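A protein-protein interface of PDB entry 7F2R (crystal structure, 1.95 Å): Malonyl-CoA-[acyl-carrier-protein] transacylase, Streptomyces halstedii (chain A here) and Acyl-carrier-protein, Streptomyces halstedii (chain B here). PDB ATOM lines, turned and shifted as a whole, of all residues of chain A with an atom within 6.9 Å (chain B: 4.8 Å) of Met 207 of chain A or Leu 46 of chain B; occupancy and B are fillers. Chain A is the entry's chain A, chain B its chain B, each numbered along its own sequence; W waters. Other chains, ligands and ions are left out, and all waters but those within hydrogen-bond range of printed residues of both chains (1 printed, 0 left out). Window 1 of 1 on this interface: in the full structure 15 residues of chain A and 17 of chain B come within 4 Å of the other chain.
Of the printed residues of chain B, Arg 154 of chain A touches Leu 46, Glu 50 and Phe 57.
Printed residues of chain A within 4 Å of Glu 50 of chain B: Arg 154 (2.9 Å).
Of the printed residues of chain A, Thr 42 of chain B touches Met 207.
Leu 209 of chain A touches none of the printed residues of chain B.
Glu 48 of chain B touches none of the printed residues of chain A.
The nearest printed residue of chain A that does not touch Leu 46 of chain B is Val 153 of chain A (6.6 Å).
The guanidinium group (NE) of Arg 154 of chain A sits at hydrogen-bond distance from the backbone carbonyl oxygen (O) of Gly 205 of chain A (2.8 Å).
O of Val 153 of chain A lies within hydrogen-bond range of N of Met 207 of chain A (3.0 Å).
The backbone NH (N) of Phe 57 of chain B is in hydrogen-bond range of the side-chain carboxylate (OE2) of Glu 50 of chain B (2.9 Å).
N of Ala 206 of chain A lies within hydrogen-bond range of O of Leu 201 of chain A, at 3.2 Å.
NH1 of Arg 154 of chain A is in hydrogen-bond range of O of Phe 57 of chain B, 3.3 Å away.
OE2 of Glu 50 of chain B is in salt-bridge range of NH1 of Arg 154 of chain A (2.9 Å).
The backbone carbonyl oxygen (O) of Pro 208 of chain A lies within hydrogen-bond range of the side-chain amino group (NZ) of Lys 64 of chain B, at 2.8 Å.
Val 153 of chain A touches Val 43 of chain B (CG2 to CG2, 3.5 Å).
Arg 154 of chain A touches Leu 46 of chain B (NH2 to CB, 3.8 Å).
Arg 202 of chain A touches Leu 62 of chain B.
Gly 205 of chain A touches Phe 57 of chain B.
Gly 205 of chain A touches Leu 62 of chain B.
Thr 42 of chain B touches Met 207 of chain A (CG2 to CE, 3.97 Å).
SD of Met 207 of chain A touches CD1 of Leu 46 of chain B (3.7 Å).
O of Leu 62 of chain B touches CG of Met 207 of chain A, 3.7 Å away.
Met 207 of chain A touches Lys 64 of chain B.
Met 207 of chain A touches Phe 67 of chain B (CE to CE2, 3.5 Å).
Of the 14 printed residues of chain A, 7 touch a printed residue of chain B.
Of the 13 printed residues of chain B, 8 touch a printed residue of chain A.
Water W1 lies within hydrogen-bond range of O of Val 43 of chain B, NH2 of Arg 154 of chain A and N of Ser 47 of chain B.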
ATOM      1  N   SER A 151     -13.160 -30.661  15.149  1.00  0.00           N
ATOM      2  CA  SER A 151     -12.825 -29.243  15.449  1.00  0.00           C
ATOM      3  C   SER A 151     -12.412 -28.578  14.123  1.00  0.00           C
ATOM      4  O   SER A 151     -11.755 -29.241  13.350  1.00  0.00           O
ATOM      5  CB  SER A 151     -11.747 -29.115  16.518  1.00  0.00           C
ATOM      6  OG  SER A 151     -10.725 -30.063  16.316  1.00  0.00           O
ATOM      7  N   PHE A 152     -12.745 -27.296  13.956  1.00  0.00           N
ATOM      8  CA  PHE A 152     -12.357 -26.463  12.795  1.00  0.00           C
ATOM      9  C   PHE A 152     -12.370 -24.999  13.174  1.00  0.00           C
ATOM     10  O   PHE A 152     -13.132 -24.552  14.089  1.00  0.00           O
ATOM     11  CB  PHE A 152     -13.290 -26.712  11.601  1.00  0.00           C
ATOM     12  CG  PHE A 152     -14.749 -26.769  11.951  1.00  0.00           C
ATOM     13  CD1 PHE A 152     -15.313 -27.944  12.406  1.00  0.00           C
ATOM     14  CD2 PHE A 152     -15.562 -25.650  11.832  1.00  0.00           C
ATOM     15  CE1 PHE A 152     -16.663 -28.004  12.722  1.00  0.00           C
ATOM     16  CE2 PHE A 152     -16.903 -25.725  12.147  1.00  0.00           C
ATOM     17  CZ  PHE A 152     -17.441 -26.872  12.637  1.00  0.00           C
ATOM     18  N   VAL A 153     -11.575 -24.243  12.428  1.00  0.00           N
ATOM     19  CA  VAL A 153     -11.345 -22.790  12.645  1.00  0.00           C
ATOM     20  C   VAL A 153     -11.585 -22.020  11.348  1.00  0.00           C
ATOM     21  O   VAL A 153     -11.950 -22.575  10.348  1.00  0.00           O
ATOM     22  CB  VAL A 153      -9.938 -22.553  13.211  1.00  0.00           C
ATOM     23  CG1 VAL A 153      -9.821 -23.157  14.573  1.00  0.00           C
ATOM     24  CG2 VAL A 153      -8.851 -23.035  12.291  1.00  0.00           C
ATOM     25  N   ARG A 154     -11.470 -20.728  11.410  1.00  0.00           N
ATOM     26  CA  ARG A 154     -11.775 -19.828  10.256  1.00  0.00           C
ATOM     27  C   ARG A 154     -13.153 -20.188   9.718  1.00  0.00           C
ATOM     28  O   ARG A 154     -13.338 -20.122   8.482  1.00  0.00           O
ATOM     29  CB  ARG A 154     -10.697 -19.966   9.173  1.00  0.00           C
ATOM     30  CG  ARG A 154      -9.308 -19.532   9.633  1.00  0.00           C
ATOM     31  CD  ARG A 154      -8.249 -20.304   8.828  1.00  0.00           C
ATOM     32  NE  ARG A 154      -8.432 -20.043   7.408  1.00  0.00           N
ATOM     33  CZ  ARG A 154      -7.887 -19.050   6.697  1.00  0.00           C
ATOM     34  NH1 ARG A 154      -8.159 -18.967   5.402  1.00  0.00           N
ATOM     35  NH2 ARG A 154      -7.095 -18.157   7.270  1.00  0.00           N
ATOM     36  N   ALA A 155     -14.090 -20.555  10.594  1.00  0.00           N
ATOM     37  CA  ALA A 155     -15.439 -20.929  10.139  1.00  0.00           C
ATOM     38  C   ALA A 155     -16.472 -20.000  10.773  1.00  0.00           C
ATOM     39  O   ALA A 155     -17.026 -20.324  11.814  1.00  0.00           O
ATOM     40  CB  ALA A 155     -15.719 -22.376  10.469  1.00  0.00           C
ATOM     41  N   GLU A 198     -14.659 -31.925   5.811  1.00  0.00           N
ATOM     42  CA  GLU A 198     -13.284 -31.364   5.719  1.00  0.00           C
ATOM     43  C   GLU A 198     -13.108 -30.630   4.386  1.00  0.00           C
ATOM     44  O   GLU A 198     -12.682 -29.464   4.414  1.00  0.00           O
ATOM     45  CB  GLU A 198     -12.296 -32.516   5.901  1.00  0.00           C
ATOM     46  CG  GLU A 198     -12.336 -33.080   7.289  1.00  0.00           C
ATOM     47  CD  GLU A 198     -11.548 -34.362   7.489  1.00  0.00           C
ATOM     48  OE1 GLU A 198     -11.158 -34.993   6.495  1.00  0.00           O
ATOM     49  OE2 GLU A 198     -11.399 -34.735   8.651  1.00  0.00           O
ATOM     50  N   LEU A 201     -15.595 -27.551   4.365  1.00  0.00           N
ATOM     51  CA  LEU A 201     -15.004 -26.442   5.182  1.00  0.00           C
ATOM     52  C   LEU A 201     -13.955 -25.690   4.338  1.00  0.00           C
ATOM     53  O   LEU A 201     -14.107 -24.447   4.122  1.00  0.00           O
ATOM     54  CB  LEU A 201     -14.395 -26.995   6.474  1.00  0.00           C
ATOM     55  CG  LEU A 201     -15.364 -27.459   7.567  1.00  0.00           C
ATOM     56  CD1 LEU A 201     -14.625 -28.346   8.572  1.00  0.00           C
ATOM     57  CD2 LEU A 201     -16.041 -26.291   8.238  1.00  0.00           C
ATOM     58  N   ARG A 202     -12.927 -26.410   3.877  1.00  0.00           N
ATOM     59  CA  ARG A 202     -11.812 -25.848   3.074  1.00  0.00           C
ATOM     60  C   ARG A 202     -12.354 -25.034   1.882  1.00  0.00           C
ATOM     61  O   ARG A 202     -11.799 -24.006   1.583  1.00  0.00           O
ATOM     62  CB  ARG A 202     -10.876 -26.965   2.609  1.00  0.00           C
ATOM     63  CG  ARG A 202     -10.002 -27.495   3.723  1.00  0.00           C
ATOM     64  CD  ARG A 202      -8.769 -28.257   3.223  1.00  0.00           C
ATOM     65  NE  ARG A 202      -9.227 -29.489   2.608  1.00  0.00           N
ATOM     66  CZ  ARG A 202      -9.392 -30.653   3.249  1.00  0.00           C
ATOM     67  NH1 ARG A 202      -9.110 -30.798   4.536  1.00  0.00           N
ATOM     68  NH2 ARG A 202      -9.862 -31.676   2.583  1.00  0.00           N
ATOM     69  N   GLY A 205     -12.798 -21.565   3.020  1.00  0.00           N
ATOM     70  CA  GLY A 205     -11.661 -20.940   3.708  1.00  0.00           C
ATOM     71  C   GLY A 205     -11.555 -21.333   5.173  1.00  0.00           C
ATOM     72  O   GLY A 205     -10.591 -20.832   5.845  1.00  0.00           O
ATOM     73  N   ALA A 206     -12.406 -22.235   5.644  1.00  0.00           N
ATOM     74  CA  ALA A 206     -12.343 -22.844   6.994  1.00  0.00           C
ATOM     75  C   ALA A 206     -11.333 -24.004   7.017  1.00  0.00           C
ATOM     76  O   ALA A 206     -11.085 -24.632   5.988  1.00  0.00           O
ATOM     77  CB  ALA A 206     -13.692 -23.292   7.392  1.00  0.00           C
ATOM     78  N   MET A 207     -10.658 -24.201   8.126  1.00  0.00           N
ATOM     79  CA  MET A 207      -9.589 -25.228   8.230  1.00  0.00           C
ATOM     80  C   MET A 207      -9.963 -26.291   9.277  1.00  0.00           C
ATOM     81  O   MET A 207     -10.034 -26.021  10.481  1.00  0.00           O
ATOM     82  CB  MET A 207      -8.242 -24.588   8.579  1.00  0.00           C
ATOM     83  CG  MET A 207      -7.093 -25.587   8.354  1.00  0.00           C
ATOM     84  SD  MET A 207      -5.527 -24.883   8.760  1.00  0.00           S
ATOM     85  CE  MET A 207      -4.446 -26.329   8.786  1.00  0.00           C
ATOM     86  N   PRO A 208     -10.145 -27.572   8.863  1.00  0.00           N
ATOM     87  CA  PRO A 208     -10.394 -28.678   9.789  1.00  0.00           C
ATOM     88  C   PRO A 208      -9.132 -28.873  10.623  1.00  0.00           C
ATOM     89  O   PRO A 208      -8.092 -28.607  10.085  1.00  0.00           O
ATOM     90  CB  PRO A 208     -10.648 -29.890   8.896  1.00  0.00           C
ATOM     91  CG  PRO A 208     -10.917 -29.279   7.541  1.00  0.00           C
ATOM     92  CD  PRO A 208     -10.038 -28.068   7.485  1.00  0.00           C
ATOM     93  N   LEU A 209      -9.280 -29.223  11.913  1.00  0.00           N
ATOM     94  CA  LEU A 209      -8.116 -29.438  12.808  1.00  0.00           C
ATOM     95  C   LEU A 209      -8.028 -30.909  13.183  1.00  0.00           C
ATOM     96  O   LEU A 209      -6.950 -31.460  12.979  1.00  0.00           O
ATOM     97  CB  LEU A 209      -8.201 -28.544  14.044  1.00  0.00           C
ATOM     98  CG  LEU A 209      -8.160 -27.041  13.785  1.00  0.00           C
ATOM     99  CD1 LEU A 209      -8.235 -26.276  15.102  1.00  0.00           C
ATOM    100  CD2 LEU A 209      -6.913 -26.632  13.004  1.00  0.00           C
ATOM    101  N   TYR A 210      -9.068 -31.479  13.791  1.00  0.00           N
ATOM    102  CA  TYR A 210      -8.991 -32.813  14.455  1.00  0.00           C
ATOM    103  C   TYR A 210     -10.390 -33.430  14.457  1.00  0.00           C
ATOM    104  O   TYR A 210     -11.422 -32.699  14.459  1.00  0.00           O
ATOM    105  CB  TYR A 210      -8.392 -32.654  15.861  1.00  0.00           C
ATOM    106  CG  TYR A 210      -7.961 -33.880  16.643  1.00  0.00           C
ATOM    107  CD1 TYR A 210      -6.714 -34.461  16.459  1.00  0.00           C
ATOM    108  CD2 TYR A 210      -8.725 -34.353  17.699  1.00  0.00           C
ATOM    109  CE1 TYR A 210      -6.277 -35.527  17.235  1.00  0.00           C
ATOM    110  CE2 TYR A 210      -8.321 -35.431  18.469  1.00  0.00           C
ATOM    111  CZ  TYR A 210      -7.088 -36.023  18.240  1.00  0.00           C
ATOM    112  OH  TYR A 210      -6.695 -37.096  18.999  1.00  0.00           O
ATOM    113  N   THR B  42      -0.722 -22.174  13.339  1.00  0.00           N
ATOM    114  CA  THR B  42      -1.105 -22.226  11.918  1.00  0.00           C
ATOM    115  C   THR B  42      -2.186 -21.185  11.649  1.00  0.00           C
ATOM    116  O   THR B  42      -2.034 -20.390  10.624  1.00  0.00           O
ATOM    117  CB  THR B  42      -1.440 -23.644  11.452  1.00  0.00           C
ATOM    118  OG1 THR B  42      -0.314 -24.481  11.741  1.00  0.00           O
ATOM    119  CG2 THR B  42      -1.716 -23.703   9.963  1.00  0.00           C
ATOM    120  N   VAL B  43      -3.207 -21.107  12.487  1.00  0.00           N
ATOM    121  CA  VAL B  43      -4.244 -20.052  12.311  1.00  0.00           C
ATOM    122  C   VAL B  43      -3.562 -18.677  12.247  1.00  0.00           C
ATOM    123  O   VAL B  43      -3.898 -17.909  11.338  1.00  0.00           O
ATOM    124  CB  VAL B  43      -5.301 -20.122  13.416  1.00  0.00           C
ATOM    125  CG1 VAL B  43      -6.347 -19.035  13.262  1.00  0.00           C
ATOM    126  CG2 VAL B  43      -5.951 -21.496  13.427  1.00  0.00           C
ATOM    127  N   GLU B  44      -2.631 -18.361  13.150  1.00  0.00           N
ATOM    128  CA  GLU B  44      -1.982 -17.025  13.225  1.00  0.00           C
ATOM    129  C   GLU B  44      -1.110 -16.813  11.983  1.00  0.00           C
ATOM    130  O   GLU B  44      -1.191 -15.727  11.379  1.00  0.00           O
ATOM    131  CB  GLU B  44      -1.117 -16.808  14.473  1.00  0.00           C
ATOM    132  CG  GLU B  44      -1.899 -16.714  15.769  1.00  0.00           C
ATOM    133  CD  GLU B  44      -3.150 -15.863  15.677  1.00  0.00           C
ATOM    134  OE1 GLU B  44      -3.020 -14.641  15.722  1.00  0.00           O
ATOM    135  OE2 GLU B  44      -4.250 -16.430  15.482  1.00  0.00           O
ATOM    136  N   LEU B  45      -0.304 -17.805  11.665  1.00  0.00           N
ATOM    137  CA  LEU B  45       0.531 -17.840  10.454  1.00  0.00           C
ATOM    138  C   LEU B  45      -0.338 -17.525   9.224  1.00  0.00           C
ATOM    139  O   LEU B  45       0.083 -16.688   8.399  1.00  0.00           O
ATOM    140  CB  LEU B  45       1.197 -19.223  10.338  1.00  0.00           C
ATOM    141  CG  LEU B  45       1.905 -19.480   9.007  1.00  0.00           C
ATOM    142  CD1 LEU B  45       3.043 -18.496   8.839  1.00  0.00           C
ATOM    143  CD2 LEU B  45       2.448 -20.895   8.947  1.00  0.00           C
ATOM    144  N   LEU B  46      -1.434 -18.254   9.051  1.00  0.00           N
ATOM    145  CA  LEU B  46      -2.347 -18.088   7.899  1.00  0.00           C
ATOM    146  C   LEU B  46      -2.833 -16.642   7.842  1.00  0.00           C
ATOM    147  O   LEU B  46      -2.794 -16.025   6.760  1.00  0.00           O
ATOM    148  CB  LEU B  46      -3.509 -19.086   8.013  1.00  0.00           C
ATOM    149  CG  LEU B  46      -3.201 -20.471   7.441  1.00  0.00           C
ATOM    150  CD1 LEU B  46      -4.309 -21.475   7.780  1.00  0.00           C
ATOM    151  CD2 LEU B  46      -2.982 -20.364   5.916  1.00  0.00           C
ATOM    152  N   SER B  47      -3.276 -16.121   8.967  1.00  0.00           N
ATOM    153  CA  SER B  47      -3.801 -14.743   9.069  1.00  0.00           C
ATOM    154  C   SER B  47      -2.696 -13.756   8.654  1.00  0.00           C
ATOM    155  O   SER B  47      -2.980 -12.757   7.945  1.00  0.00           O
ATOM    156  CB  SER B  47      -4.347 -14.498  10.462  1.00  0.00           C
ATOM    157  OG  SER B  47      -4.737 -13.156  10.588  1.00  0.00           O
ATOM    158  N   GLU B  48      -1.450 -14.023   9.041  1.00  0.00           N
ATOM    159  CA  GLU B  48      -0.334 -13.110   8.713  1.00  0.00           C
ATOM    160  C   GLU B  48       0.016 -13.283   7.238  1.00  0.00           C
ATOM    161  O   GLU B  48       0.272 -12.253   6.568  1.00  0.00           O
ATOM    162  CB  GLU B  48       0.892 -13.307   9.606  1.00  0.00           C
ATOM    163  CG  GLU B  48       1.845 -12.128   9.481  1.00  0.00           C
ATOM    164  CD  GLU B  48       2.915 -12.024  10.540  1.00  0.00           C
ATOM    165  OE1 GLU B  48       2.907 -12.831  11.497  1.00  0.00           O
ATOM    166  OE2 GLU B  48       3.736 -11.136  10.418  1.00  0.00           O
ATOM    167  N   LEU B  49       0.042 -14.508   6.724  1.00  0.00           N
ATOM    168  CA  LEU B  49       0.379 -14.728   5.293  1.00  0.00           C
ATOM    169  C   LEU B  49      -0.681 -14.049   4.422  1.00  0.00           C
ATOM    170  O   LEU B  49      -0.311 -13.484   3.368  1.00  0.00           O
ATOM    171  CB  LEU B  49       0.405 -16.213   5.004  1.00  0.00           C
ATOM    172  CG  LEU B  49       1.638 -16.957   5.497  1.00  0.00           C
ATOM    173  CD1 LEU B  49       1.411 -18.441   5.309  1.00  0.00           C
ATOM    174  CD2 LEU B  49       2.915 -16.479   4.809  1.00  0.00           C
ATOM    175  N   GLU B  50      -1.955 -14.138   4.822  1.00  0.00           N
ATOM    176  CA  GLU B  50      -3.066 -13.609   3.999  1.00  0.00           C
ATOM    177  C   GLU B  50      -2.999 -12.092   4.004  1.00  0.00           C
ATOM    178  O   GLU B  50      -3.100 -11.553   2.929  1.00  0.00           O
ATOM    179  CB  GLU B  50      -4.399 -14.168   4.447  1.00  0.00           C
ATOM    180  CG  GLU B  50      -4.565 -15.638   4.117  1.00  0.00           C
ATOM    181  CD  GLU B  50      -5.880 -16.218   4.602  1.00  0.00           C
ATOM    182  OE1 GLU B  50      -6.419 -15.675   5.610  1.00  0.00           O
ATOM    183  OE2 GLU B  50      -6.335 -17.209   4.007  1.00  0.00           O
ATOM    184  N   PHE B  57      -6.149 -18.350   1.401  1.00  0.00           N
ATOM    185  CA  PHE B  57      -5.924 -19.803   1.372  1.00  0.00           C
ATOM    186  C   PHE B  57      -7.300 -20.481   1.418  1.00  0.00           C
ATOM    187  O   PHE B  57      -8.056 -20.273   2.370  1.00  0.00           O
ATOM    188  CB  PHE B  57      -5.050 -20.262   2.539  1.00  0.00           C
ATOM    189  CG  PHE B  57      -3.573 -20.006   2.440  1.00  0.00           C
ATOM    190  CD1 PHE B  57      -3.061 -18.726   2.454  1.00  0.00           C
ATOM    191  CD2 PHE B  57      -2.688 -21.059   2.434  1.00  0.00           C
ATOM    192  CE1 PHE B  57      -1.697 -18.510   2.403  1.00  0.00           C
ATOM    193  CE2 PHE B  57      -1.318 -20.848   2.388  1.00  0.00           C
ATOM    194  CZ  PHE B  57      -0.820 -19.571   2.334  1.00  0.00           C
ATOM    195  N   LEU B  62      -5.501 -25.457   2.106  1.00  0.00           N
ATOM    196  CA  LEU B  62      -5.800 -25.589   3.553  1.00  0.00           C
ATOM    197  C   LEU B  62      -5.626 -27.020   4.051  1.00  0.00           C
ATOM    198  O   LEU B  62      -5.879 -27.228   5.261  1.00  0.00           O
ATOM    199  CB  LEU B  62      -7.197 -25.034   3.838  1.00  0.00           C
ATOM    200  CG  LEU B  62      -7.261 -23.518   3.828  1.00  0.00           C
ATOM    201  CD1 LEU B  62      -8.676 -23.059   4.070  1.00  0.00           C
ATOM    202  CD2 LEU B  62      -6.307 -22.928   4.877  1.00  0.00           C
ATOM    203  N   LYS B  64      -3.477 -30.217   5.489  1.00  0.00           N
ATOM    204  CA  LYS B  64      -2.308 -30.467   6.378  1.00  0.00           C
ATOM    205  C   LYS B  64      -1.021 -30.402   5.571  1.00  0.00           C
ATOM    206  O   LYS B  64      -0.045 -29.868   6.113  1.00  0.00           O
ATOM    207  CB  LYS B  64      -2.398 -31.853   7.023  1.00  0.00           C
ATOM    208  CG  LYS B  64      -3.720 -32.128   7.729  1.00  0.00           C
ATOM    209  CD  LYS B  64      -4.343 -30.894   8.449  1.00  0.00           C
ATOM    210  CE  LYS B  64      -5.862 -30.891   8.584  1.00  0.00           C
ATOM    211  NZ  LYS B  64      -6.470 -29.616   8.103  1.00  0.00           N
ATOM    212  N   PHE B  67       1.227 -27.255   5.171  1.00  0.00           N
ATOM    213  CA  PHE B  67       2.048 -26.772   6.316  1.00  0.00           C
ATOM    214  C   PHE B  67       3.044 -27.831   6.785  1.00  0.00           C
ATOM    215  O   PHE B  67       3.642 -27.671   7.865  1.00  0.00           O
ATOM    216  CB  PHE B  67       1.147 -26.332   7.454  1.00  0.00           C
ATOM    217  CG  PHE B  67       0.036 -25.459   6.943  1.00  0.00           C
ATOM    218  CD1 PHE B  67       0.280 -24.143   6.601  1.00  0.00           C
ATOM    219  CD2 PHE B  67      -1.234 -25.976   6.746  1.00  0.00           C
ATOM    220  CE1 PHE B  67      -0.738 -23.350   6.096  1.00  0.00           C
ATOM    221  CE2 PHE B  67      -2.255 -25.180   6.253  1.00  0.00           C
ATOM    222  CZ  PHE B  67      -1.993 -23.886   5.895  1.00  0.00           C
HETATM  223  O   HOH W   1      -6.146 -17.835   9.992  1.00  0.00           O
